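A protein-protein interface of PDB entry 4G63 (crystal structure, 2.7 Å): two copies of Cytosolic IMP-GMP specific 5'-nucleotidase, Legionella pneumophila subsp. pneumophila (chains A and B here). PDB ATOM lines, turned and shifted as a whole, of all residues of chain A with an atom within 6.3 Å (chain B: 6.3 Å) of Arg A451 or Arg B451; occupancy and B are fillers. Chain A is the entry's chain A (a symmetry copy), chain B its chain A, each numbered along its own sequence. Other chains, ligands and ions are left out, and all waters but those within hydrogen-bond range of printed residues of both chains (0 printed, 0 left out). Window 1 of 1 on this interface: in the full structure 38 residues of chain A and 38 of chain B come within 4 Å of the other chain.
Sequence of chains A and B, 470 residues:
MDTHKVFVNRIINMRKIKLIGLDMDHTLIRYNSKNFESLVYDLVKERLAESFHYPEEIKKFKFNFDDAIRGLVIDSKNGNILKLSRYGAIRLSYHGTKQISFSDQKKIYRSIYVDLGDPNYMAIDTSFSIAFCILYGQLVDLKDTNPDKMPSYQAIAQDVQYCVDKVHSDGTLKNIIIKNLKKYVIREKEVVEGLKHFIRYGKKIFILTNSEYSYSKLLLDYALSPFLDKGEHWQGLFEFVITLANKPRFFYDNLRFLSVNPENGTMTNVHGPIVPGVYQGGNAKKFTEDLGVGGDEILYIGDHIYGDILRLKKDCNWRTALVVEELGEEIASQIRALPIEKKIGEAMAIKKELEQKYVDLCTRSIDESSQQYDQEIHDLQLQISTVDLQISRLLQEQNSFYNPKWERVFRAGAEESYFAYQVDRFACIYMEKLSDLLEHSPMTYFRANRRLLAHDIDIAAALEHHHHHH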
ATOM      1  N   ARG A  86      13.103  34.869  19.127  1.00  0.00           N
ATOM      2  CA  ARG A  86      12.107  34.006  18.513  1.00  0.00           C
ATOM      3  C   ARG A  86      11.454  34.660  17.293  1.00  0.00           C
ATOM      4  O   ARG A  86      11.104  33.976  16.343  1.00  0.00           O
ATOM      5  CB  ARG A  86      11.042  33.639  19.556  1.00  0.00           C
ATOM      6  CG  ARG A  86       9.843  32.857  19.029  1.00  0.00           C
ATOM      7  CD  ARG A  86       8.803  32.646  20.135  1.00  0.00           C
ATOM      8  NE  ARG A  86       8.493  33.907  20.813  1.00  0.00           N
ATOM      9  CZ  ARG A  86       7.633  34.039  21.824  1.00  0.00           C
ATOM     10  NH1 ARG A  86       6.981  32.979  22.293  1.00  0.00           N
ATOM     11  NH2 ARG A  86       7.426  35.238  22.366  1.00  0.00           N
ATOM     12  N   ARG A 411      17.981  31.054  25.045  1.00  0.00           N
ATOM     13  CA  ARG A 411      17.492  32.363  25.444  1.00  0.00           C
ATOM     14  C   ARG A 411      18.166  33.460  24.642  1.00  0.00           C
ATOM     15  O   ARG A 411      19.349  33.384  24.353  1.00  0.00           O
ATOM     16  CB  ARG A 411      17.764  32.592  26.934  1.00  0.00           C
ATOM     17  CG  ARG A 411      16.933  31.753  27.863  1.00  0.00           C
ATOM     18  CD  ARG A 411      15.550  32.321  27.990  1.00  0.00           C
ATOM     19  NE  ARG A 411      14.676  31.397  28.695  1.00  0.00           N
ATOM     20  CZ  ARG A 411      13.407  31.652  28.984  1.00  0.00           C
ATOM     21  NH1 ARG A 411      12.868  32.807  28.633  1.00  0.00           N
ATOM     22  NH2 ARG A 411      12.667  30.745  29.603  1.00  0.00           N
ATOM     23  N   ALA A 414      15.727  37.989  27.425  1.00  0.00           N
ATOM     24  CA  ALA A 414      14.888  37.253  28.371  1.00  0.00           C
ATOM     25  C   ALA A 414      13.881  36.298  27.739  1.00  0.00           C
ATOM     26  O   ALA A 414      13.293  35.479  28.435  1.00  0.00           O
ATOM     27  CB  ALA A 414      14.149  38.238  29.266  1.00  0.00           C
ATOM     28  N   GLU A 415      13.668  36.405  26.430  1.00  0.00           N
ATOM     29  CA  GLU A 415      12.704  35.544  25.742  1.00  0.00           C
ATOM     30  C   GLU A 415      13.423  34.408  25.034  1.00  0.00           C
ATOM     31  O   GLU A 415      14.654  34.375  25.019  1.00  0.00           O
ATOM     32  CB  GLU A 415      11.915  36.369  24.725  1.00  0.00           C
ATOM     33  CG  GLU A 415      12.734  36.838  23.539  1.00  0.00           C
ATOM     34  CD  GLU A 415      12.234  38.157  22.973  1.00  0.00           C
ATOM     35  OE1 GLU A 415      11.001  38.313  22.818  1.00  0.00           O
ATOM     36  OE2 GLU A 415      13.082  39.034  22.676  1.00  0.00           O
ATOM     37  N   GLU A 416      12.670  33.481  24.445  1.00  0.00           N
ATOM     38  CA  GLU A 416      13.314  32.383  23.741  1.00  0.00           C
ATOM     39  C   GLU A 416      14.052  32.858  22.487  1.00  0.00           C
ATOM     40  O   GLU A 416      13.580  33.732  21.762  1.00  0.00           O
ATOM     41  CB  GLU A 416      12.313  31.281  23.374  1.00  0.00           C
ATOM     42  CG  GLU A 416      11.019  31.729  22.762  1.00  0.00           C
ATOM     43  CD  GLU A 416       9.969  32.019  23.807  1.00  0.00           C
ATOM     44  OE1 GLU A 416       9.943  33.158  24.347  1.00  0.00           O
ATOM     45  OE2 GLU A 416       9.177  31.095  24.093  1.00  0.00           O
ATOM     46  N   ASP A 424      11.218  24.133  19.096  1.00  0.00           N
ATOM     47  CA  ASP A 424       9.799  24.081  19.392  1.00  0.00           C
ATOM     48  C   ASP A 424       8.934  23.721  18.180  1.00  0.00           C
ATOM     49  O   ASP A 424       8.035  22.881  18.270  1.00  0.00           O
ATOM     50  CB  ASP A 424       9.359  25.440  19.948  1.00  0.00           C
ATOM     51  CG  ASP A 424       7.932  25.437  20.474  1.00  0.00           C
ATOM     52  OD1 ASP A 424       7.246  26.467  20.309  1.00  0.00           O
ATOM     53  OD2 ASP A 424       7.496  24.425  21.066  1.00  0.00           O
ATOM     54  N   ASN A 449       3.325  20.332  28.623  1.00  0.00           N
ATOM     55  CA  ASN A 449       2.708  21.151  29.660  1.00  0.00           C
ATOM     56  C   ASN A 449       1.835  22.226  29.039  1.00  0.00           C
ATOM     57  O   ASN A 449       2.099  22.683  27.927  1.00  0.00           O
ATOM     58  CB  ASN A 449       3.778  21.824  30.504  1.00  0.00           C
ATOM     59  CG  ASN A 449       4.713  20.833  31.139  1.00  0.00           C
ATOM     60  OD1 ASN A 449       4.301  20.029  31.975  1.00  0.00           O
ATOM     61  ND2 ASN A 449       5.981  20.870  30.740  1.00  0.00           N
ATOM     62  N   ARG A 450       0.794  22.629  29.763  1.00  0.00           N
ATOM     63  CA  ARG A 450      -0.116  23.669  29.286  1.00  0.00           C
ATOM     64  C   ARG A 450       0.719  24.933  29.158  1.00  0.00           C
ATOM     65  O   ARG A 450       1.369  25.338  30.113  1.00  0.00           O
ATOM     66  CB  ARG A 450      -1.237  23.882  30.307  1.00  0.00           C
ATOM     67  CG  ARG A 450      -2.632  24.097  29.721  1.00  0.00           C
ATOM     68  CD  ARG A 450      -2.719  25.367  28.893  1.00  0.00           C
ATOM     69  NE  ARG A 450      -4.088  25.883  28.814  1.00  0.00           N
ATOM     70  CZ  ARG A 450      -5.118  25.241  28.264  1.00  0.00           C
ATOM     71  NH1 ARG A 450      -4.953  24.034  27.731  1.00  0.00           N
ATOM     72  NH2 ARG A 450      -6.317  25.814  28.243  1.00  0.00           N
ATOM     73  N   ARG A 451       0.705  25.555  27.985  1.00  0.00           N
ATOM     74  CA  ARG A 451       1.502  26.756  27.762  1.00  0.00           C
ATOM     75  C   ARG A 451       1.106  27.920  28.668  1.00  0.00           C
ATOM     76  O   ARG A 451       1.961  28.482  29.358  1.00  0.00           O
ATOM     77  CB  ARG A 451       1.419  27.179  26.291  1.00  0.00           C
ATOM     78  CG  ARG A 451       2.623  27.991  25.781  1.00  0.00           C
ATOM     79  CD  ARG A 451       2.796  29.347  26.496  1.00  0.00           C
ATOM     80  NE  ARG A 451       3.800  30.195  25.843  1.00  0.00           N
ATOM     81  CZ  ARG A 451       4.049  31.465  26.163  1.00  0.00           C
ATOM     82  NH1 ARG A 451       3.366  32.059  27.140  1.00  0.00           N
ATOM     83  NH2 ARG A 451       4.980  32.146  25.496  1.00  0.00           N
ATOM     84  N   LEU A 452      -0.175  28.282  28.659  1.00  0.00           N
ATOM     85  CA  LEU A 452      -0.712  29.383  29.478  1.00  0.00           C
ATOM     86  C   LEU A 452      -0.430  30.802  28.955  1.00  0.00           C
ATOM     87  O   LEU A 452       0.710  31.269  28.946  1.00  0.00           O
ATOM     88  CB  LEU A 452      -0.231  29.275  30.931  1.00  0.00           C
ATOM     89  CG  LEU A 452      -1.338  29.425  31.991  1.00  0.00           C
ATOM     90  CD1 LEU A 452      -2.139  28.139  32.073  1.00  0.00           C
ATOM     91  CD2 LEU A 452      -0.735  29.747  33.352  1.00  0.00           C
ATOM     92  N   LEU A 453      -1.496  31.484  28.539  1.00  0.00           N
ATOM     93  CA  LEU A 453      -1.415  32.839  28.005  1.00  0.00           C
ATOM     94  C   LEU A 453      -1.463  33.911  29.089  1.00  0.00           C
ATOM     95  O   LEU A 453      -1.855  33.652  30.230  1.00  0.00           O
ATOM     96  CB  LEU A 453      -2.549  33.060  27.008  1.00  0.00           C
ATOM     97  CG  LEU A 453      -2.608  32.001  25.904  1.00  0.00           C
ATOM     98  CD1 LEU A 453      -3.789  32.280  24.985  1.00  0.00           C
ATOM     99  CD2 LEU A 453      -1.298  31.996  25.124  1.00  0.00           C
ATOM    100  N   ALA A 454      -1.073  35.124  28.719  1.00  0.00           N
ATOM    101  CA  ALA A 454      -1.038  36.234  29.659  1.00  0.00           C
ATOM    102  C   ALA A 454      -2.377  36.540  30.320  1.00  0.00           C
ATOM    103  O   ALA A 454      -2.418  37.049  31.435  1.00  0.00           O
ATOM    104  CB  ALA A 454      -0.501  37.479  28.965  1.00  0.00           C
ATOM    105  N   ASP A 456      -4.670  34.241  31.053  1.00  0.00           N
ATOM    106  CA  ASP A 456      -5.158  33.004  31.672  1.00  0.00           C
ATOM    107  C   ASP A 456      -4.983  33.080  33.190  1.00  0.00           C
ATOM    108  O   ASP A 456      -4.047  33.722  33.683  1.00  0.00           O
ATOM    109  CB  ASP A 456      -4.382  31.781  31.168  1.00  0.00           C
ATOM    110  CG  ASP A 456      -4.782  31.356  29.771  1.00  0.00           C
ATOM    111  OD1 ASP A 456      -5.907  31.682  29.352  1.00  0.00           O
ATOM    112  OD2 ASP A 456      -3.978  30.672  29.098  1.00  0.00           O
ATOM    113  N   ARG B  86      -0.747  27.951  16.221  1.00  0.00           N
ATOM    114  CA  ARG B  86       0.333  28.922  16.172  1.00  0.00           C
ATOM    115  C   ARG B  86       1.292  28.660  15.009  1.00  0.00           C
ATOM    116  O   ARG B  86       1.836  29.594  14.438  1.00  0.00           O
ATOM    117  CB  ARG B  86       1.094  28.900  17.506  1.00  0.00           C
ATOM    118  CG  ARG B  86       2.354  29.759  17.563  1.00  0.00           C
ATOM    119  CD  ARG B  86       3.082  29.569  18.898  1.00  0.00           C
ATOM    120  NE  ARG B  86       3.267  28.147  19.199  1.00  0.00           N
ATOM    121  CZ  ARG B  86       3.856  27.670  20.295  1.00  0.00           C
ATOM    122  NH1 ARG B  86       4.330  28.502  21.220  1.00  0.00           N
ATOM    123  NH2 ARG B  86       3.972  26.354  20.466  1.00  0.00           N
ATOM    124  N   ARG B 411      -7.077  29.904  21.651  1.00  0.00           N
ATOM    125  CA  ARG B 411      -6.648  28.517  21.726  1.00  0.00           C
ATOM    126  C   ARG B 411      -7.060  27.756  20.480  1.00  0.00           C
ATOM    127  O   ARG B 411      -8.139  27.966  19.949  1.00  0.00           O
ATOM    128  CB  ARG B 411      -7.268  27.842  22.953  1.00  0.00           C
ATOM    129  CG  ARG B 411      -6.724  28.312  24.273  1.00  0.00           C
ATOM    130  CD  ARG B 411      -5.393  27.678  24.550  1.00  0.00           C
ATOM    131  NE  ARG B 411      -4.757  28.297  25.701  1.00  0.00           N
ATOM    132  CZ  ARG B 411      -3.587  27.913  26.197  1.00  0.00           C
ATOM    133  NH1 ARG B 411      -2.933  26.906  25.644  1.00  0.00           N
ATOM    134  NH2 ARG B 411      -3.060  28.549  27.232  1.00  0.00           N
ATOM    135  N   ALA B 414      -5.198  22.487  22.205  1.00  0.00           N
ATOM    136  CA  ALA B 414      -4.647  22.853  23.510  1.00  0.00           C
ATOM    137  C   ALA B 414      -3.555  23.918  23.478  1.00  0.00           C
ATOM    138  O   ALA B 414      -3.189  24.452  24.517  1.00  0.00           O
ATOM    139  CB  ALA B 414      -4.111  21.608  24.202  1.00  0.00           C
ATOM    140  N   GLU B 415      -3.023  24.219  22.296  1.00  0.00           N
ATOM    141  CA  GLU B 415      -1.956  25.214  22.172  1.00  0.00           C
ATOM    142  C   GLU B 415      -2.524  26.543  21.704  1.00  0.00           C
ATOM    143  O   GLU B 415      -3.714  26.628  21.399  1.00  0.00           O
ATOM    144  CB  GLU B 415      -0.908  24.720  21.174  1.00  0.00           C
ATOM    145  CG  GLU B 415      -1.392  24.681  19.737  1.00  0.00           C
ATOM    146  CD  GLU B 415      -0.716  23.588  18.926  1.00  0.00           C
ATOM    147  OE1 GLU B 415       0.523  23.439  19.037  1.00  0.00           O
ATOM    148  OE2 GLU B 415      -1.429  22.884  18.170  1.00  0.00           O
ATOM    149  N   GLU B 416      -1.688  27.577  21.640  1.00  0.00           N
ATOM    150  CA  GLU B 416      -2.182  28.866  21.183  1.00  0.00           C
ATOM    151  C   GLU B 416      -2.571  28.840  19.702  1.00  0.00           C
ATOM    152  O   GLU B 416      -1.901  28.220  18.878  1.00  0.00           O
ATOM    153  CB  GLU B 416      -1.167  29.985  21.438  1.00  0.00           C
ATOM    154  CG  GLU B 416       0.254  29.702  21.053  1.00  0.00           C
ATOM    155  CD  GLU B 416       1.027  29.055  22.177  1.00  0.00           C
ATOM    156  OE1 GLU B 416       0.965  27.804  22.320  1.00  0.00           O
ATOM    157  OE2 GLU B 416       1.686  29.810  22.924  1.00  0.00           O
ATOM    158  N   ASP B 424       0.654  38.067  20.031  1.00  0.00           N
ATOM    159  CA  ASP B 424       1.954  37.966  20.668  1.00  0.00           C
ATOM    160  C   ASP B 424       3.075  38.653  19.882  1.00  0.00           C
ATOM    161  O   ASP B 424       3.889  39.386  20.448  1.00  0.00           O
ATOM    162  CB  ASP B 424       2.298  36.484  20.858  1.00  0.00           C
ATOM    163  CG  ASP B 424       3.552  36.265  21.691  1.00  0.00           C
ATOM    164  OD1 ASP B 424       4.298  35.311  21.383  1.00  0.00           O
ATOM    165  OD2 ASP B 424       3.788  37.020  22.659  1.00  0.00           O
ATOM    166  N   ASN B 449       5.812  38.357  31.899  1.00  0.00           N
ATOM    167  CA  ASN B 449       6.187  37.229  32.743  1.00  0.00           C
ATOM    168  C   ASN B 449       7.229  36.369  32.050  1.00  0.00           C
ATOM    169  O   ASN B 449       7.264  36.296  30.822  1.00  0.00           O
ATOM    170  CB  ASN B 449       4.971  36.368  33.044  1.00  0.00           C
ATOM    171  CG  ASN B 449       3.870  37.146  33.709  1.00  0.00           C
ATOM    172  OD1 ASN B 449       4.032  37.629  34.829  1.00  0.00           O
ATOM    173  ND2 ASN B 449       2.741  37.287  33.020  1.00  0.00           N
ATOM    174  N   ARG B 450       8.076  35.718  32.842  1.00  0.00           N
ATOM    175  CA  ARG B 450       9.116  34.845  32.301  1.00  0.00           C
ATOM    176  C   ARG B 450       8.390  33.720  31.581  1.00  0.00           C
ATOM    177  O   ARG B 450       7.542  33.062  32.170  1.00  0.00           O
ATOM    178  CB  ARG B 450       9.960  34.277  33.445  1.00  0.00           C
ATOM    179  CG  ARG B 450      11.464  34.201  33.182  1.00  0.00           C
ATOM    180  CD  ARG B 450      11.802  33.254  32.045  1.00  0.00           C
ATOM    181  NE  ARG B 450      13.168  32.734  32.146  1.00  0.00           N
ATOM    182  CZ  ARG B 450      14.275  33.475  32.095  1.00  0.00           C
ATOM    183  NH1 ARG B 450      14.197  34.793  31.946  1.00  0.00           N
ATOM    184  NH2 ARG B 450      15.465  32.889  32.190  1.00  0.00           N
ATOM    185  N   ARG B 451       8.716  33.499  30.313  1.00  0.00           N
ATOM    186  CA  ARG B 451       8.046  32.462  29.535  1.00  0.00           C
ATOM    187  C   ARG B 451       8.255  31.057  30.097  1.00  0.00           C
ATOM    188  O   ARG B 451       7.280  30.341  30.343  1.00  0.00           O
ATOM    189  CB  ARG B 451       8.505  32.520  28.073  1.00  0.00           C
ATOM    190  CG  ARG B 451       7.497  31.959  27.056  1.00  0.00           C
ATOM    191  CD  ARG B 451       7.208  30.455  27.242  1.00  0.00           C
ATOM    192  NE  ARG B 451       6.430  29.896  26.131  1.00  0.00           N
ATOM    193  CZ  ARG B 451       6.161  28.601  25.963  1.00  0.00           C
ATOM    194  NH1 ARG B 451       6.607  27.703  26.840  1.00  0.00           N
ATOM    195  NH2 ARG B 451       5.450  28.203  24.908  1.00  0.00           N
ATOM    196  N   LEU B 452       9.513  30.665  30.289  1.00  0.00           N
ATOM    197  CA  LEU B 452       9.876  29.342  30.825  1.00  0.00           C
ATOM    198  C   LEU B 452       9.788  28.172  29.831  1.00  0.00           C
ATOM    199  O   LEU B 452       8.705  27.778  29.396  1.00  0.00           O
ATOM    200  CB  LEU B 452       9.050  29.006  32.074  1.00  0.00           C
ATOM    201  CG  LEU B 452       9.868  28.486  33.270  1.00  0.00           C
ATOM    202  CD1 LEU B 452      10.573  29.648  33.946  1.00  0.00           C
ATOM    203  CD2 LEU B 452       8.964  27.776  34.269  1.00  0.00           C
ATOM    204  N   LEU B 453      10.950  27.613  29.495  1.00  0.00           N
ATOM    205  CA  LEU B 453      11.057  26.500  28.559  1.00  0.00           C
ATOM    206  C   LEU B 453      10.881  25.140  29.229  1.00  0.00           C
ATOM    207  O   LEU B 453      10.971  25.010  30.452  1.00  0.00           O
ATOM    208  CB  LEU B 453      12.409  26.557  27.854  1.00  0.00           C
ATOM    209  CG  LEU B 453      12.694  27.907  27.189  1.00  0.00           C
ATOM    210  CD1 LEU B 453      14.075  27.884  26.549  1.00  0.00           C
ATOM    211  CD2 LEU B 453      11.616  28.209  26.155  1.00  0.00           C
ATOM    212  N   ALA B 454      10.643  24.121  28.412  1.00  0.00           N
ATOM    213  CA  ALA B 454      10.423  22.774  28.916  1.00  0.00           C
ATOM    214  C   ALA B 454      11.571  22.222  29.754  1.00  0.00           C
ATOM    215  O   ALA B 454      11.357  21.387  30.627  1.00  0.00           O
ATOM    216  CB  ALA B 454      10.123  21.833  27.756  1.00  0.00           C
ATOM    217  N   ASP B 456      13.519  24.079  31.712  1.00  0.00           N
ATOM    218  CA  ASP B 456      13.791  25.038  32.788  1.00  0.00           C
ATOM    219  C   ASP B 456      13.252  24.496  34.113  1.00  0.00           C
ATOM    220  O   ASP B 456      12.250  23.769  34.134  1.00  0.00           O
ATOM    221  CB  ASP B 456      13.113  26.388  32.521  1.00  0.00           C
ATOM    222  CG  ASP B 456      13.826  27.214  31.471  1.00  0.00           C
ATOM    223  OD1 ASP B 456      15.032  26.991  31.260  1.00  0.00           O
ATOM    224  OD2 ASP B 456      13.185  28.107  30.872  1.00  0.00           O
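The backbone NH of Leu A452 sits close to the guanidinium group of Arg B411 (3.2 Å).
OE2 of Glu B416 lies within salt-bridge range of NE of Arg A451.
The side-chain carboxylate of Asp A456 is in salt-bridge range of the guanidinium group of Arg B411 (3.0 Å).
The guanidinium group of Arg A411 lies within salt-bridge range of the side-chain carboxylate of Asp B456 (3.0 Å).
NH2 of Arg A411 sits close to N of Leu B452, 3.2 Å away.
NE of Arg B450 lies close to NH2 of Arg A411 (3.3 Å).
The side-chain carboxylate (OD1) of Asp B424 is in salt-bridge range of the guanidinium group (NH2) of Arg A86 (3.3 Å).
The guanidinium group of Arg B451 sits close to the guanidinium group of Arg A451, 2.7 Å away.
OD1 of Asp A424 is in salt-bridge range of NH2 of Arg B86 (3.3 Å).
NH2 of Arg B411 lies close to NE of Arg A450 (3.3 Å).
NE of Arg B451 is in salt-bridge range of OE2 of Glu A416, at 3.6 Å.
The side-chain carboxylate of Glu B416 is in salt-bridge range of the guanidinium group of Arg B86, 3.4 Å away.
NH1 of Arg B411 sits at hydrogen-bond distance from O of Ala B414 (2.7 Å).
The side-chain carboxylate (OD2) of Asp A456 is in hydrogen-bond range of the backbone NH (N) of Leu A453 (2.7 Å).
N of Leu B453 lies within hydrogen-bond range of OD2 of Asp B456 (2.7 Å).
The guanidinium group (NH1) of Arg A411 sits at hydrogen-bond distance from the backbone carbonyl oxygen (O) of Ala A414, at 2.7 Å.
The guanidinium group of Arg A86 is in salt-bridge range of the side-chain carboxylate of Glu A416, 3.4 Å away.
NH2 of Arg A411 touches N of Leu B453 (3.6 Å).
NH1 of Arg B450 touches O of Ala A414, at 3.7 Å.
NH1 of Arg A450 touches O of Ala B414, at 3.7 Å.
NH2 of Arg B411 touches N of Leu A453, 3.6 Å away.
Of the printed residues of chain B, Arg A451 touches Glu B416 (3.5 Å) and Arg B451 (2.7 Å).
Of chain A, only Glu A416 (3.5 Å) and Arg A451 (2.7 Å) come within 4 Å of Arg B451.
Of the printed residues of chain A, Asp B424 touches Arg A86 (3.3 Å).
Of the printed residues of chain A, Glu B416 touches Arg A451.
Glu A415 touches none of the printed residues of chain B.
The nearest residue of chain A that does not touch Arg B451 is Arg A411 (4.4 Å).
Hydrophobic or aromatic side chains of chain A within 4 Å of the printed part of chain B: Leu A453.
Among the printed residues, 15 pairs touch across the chains.
Arg A86 touches Asp B424, and with the chains exchanged Asp A424 touches Arg B86.
Arg A411 touches Leu B453, and with the chains exchanged Leu A453 touches Arg B411.
Arg A411 touches Asp B456, and with the chains exchanged Asp A456 touches Arg B411.
Arg B451 touches its own counterpart, Arg A451.
13 positions are printed for both chains.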
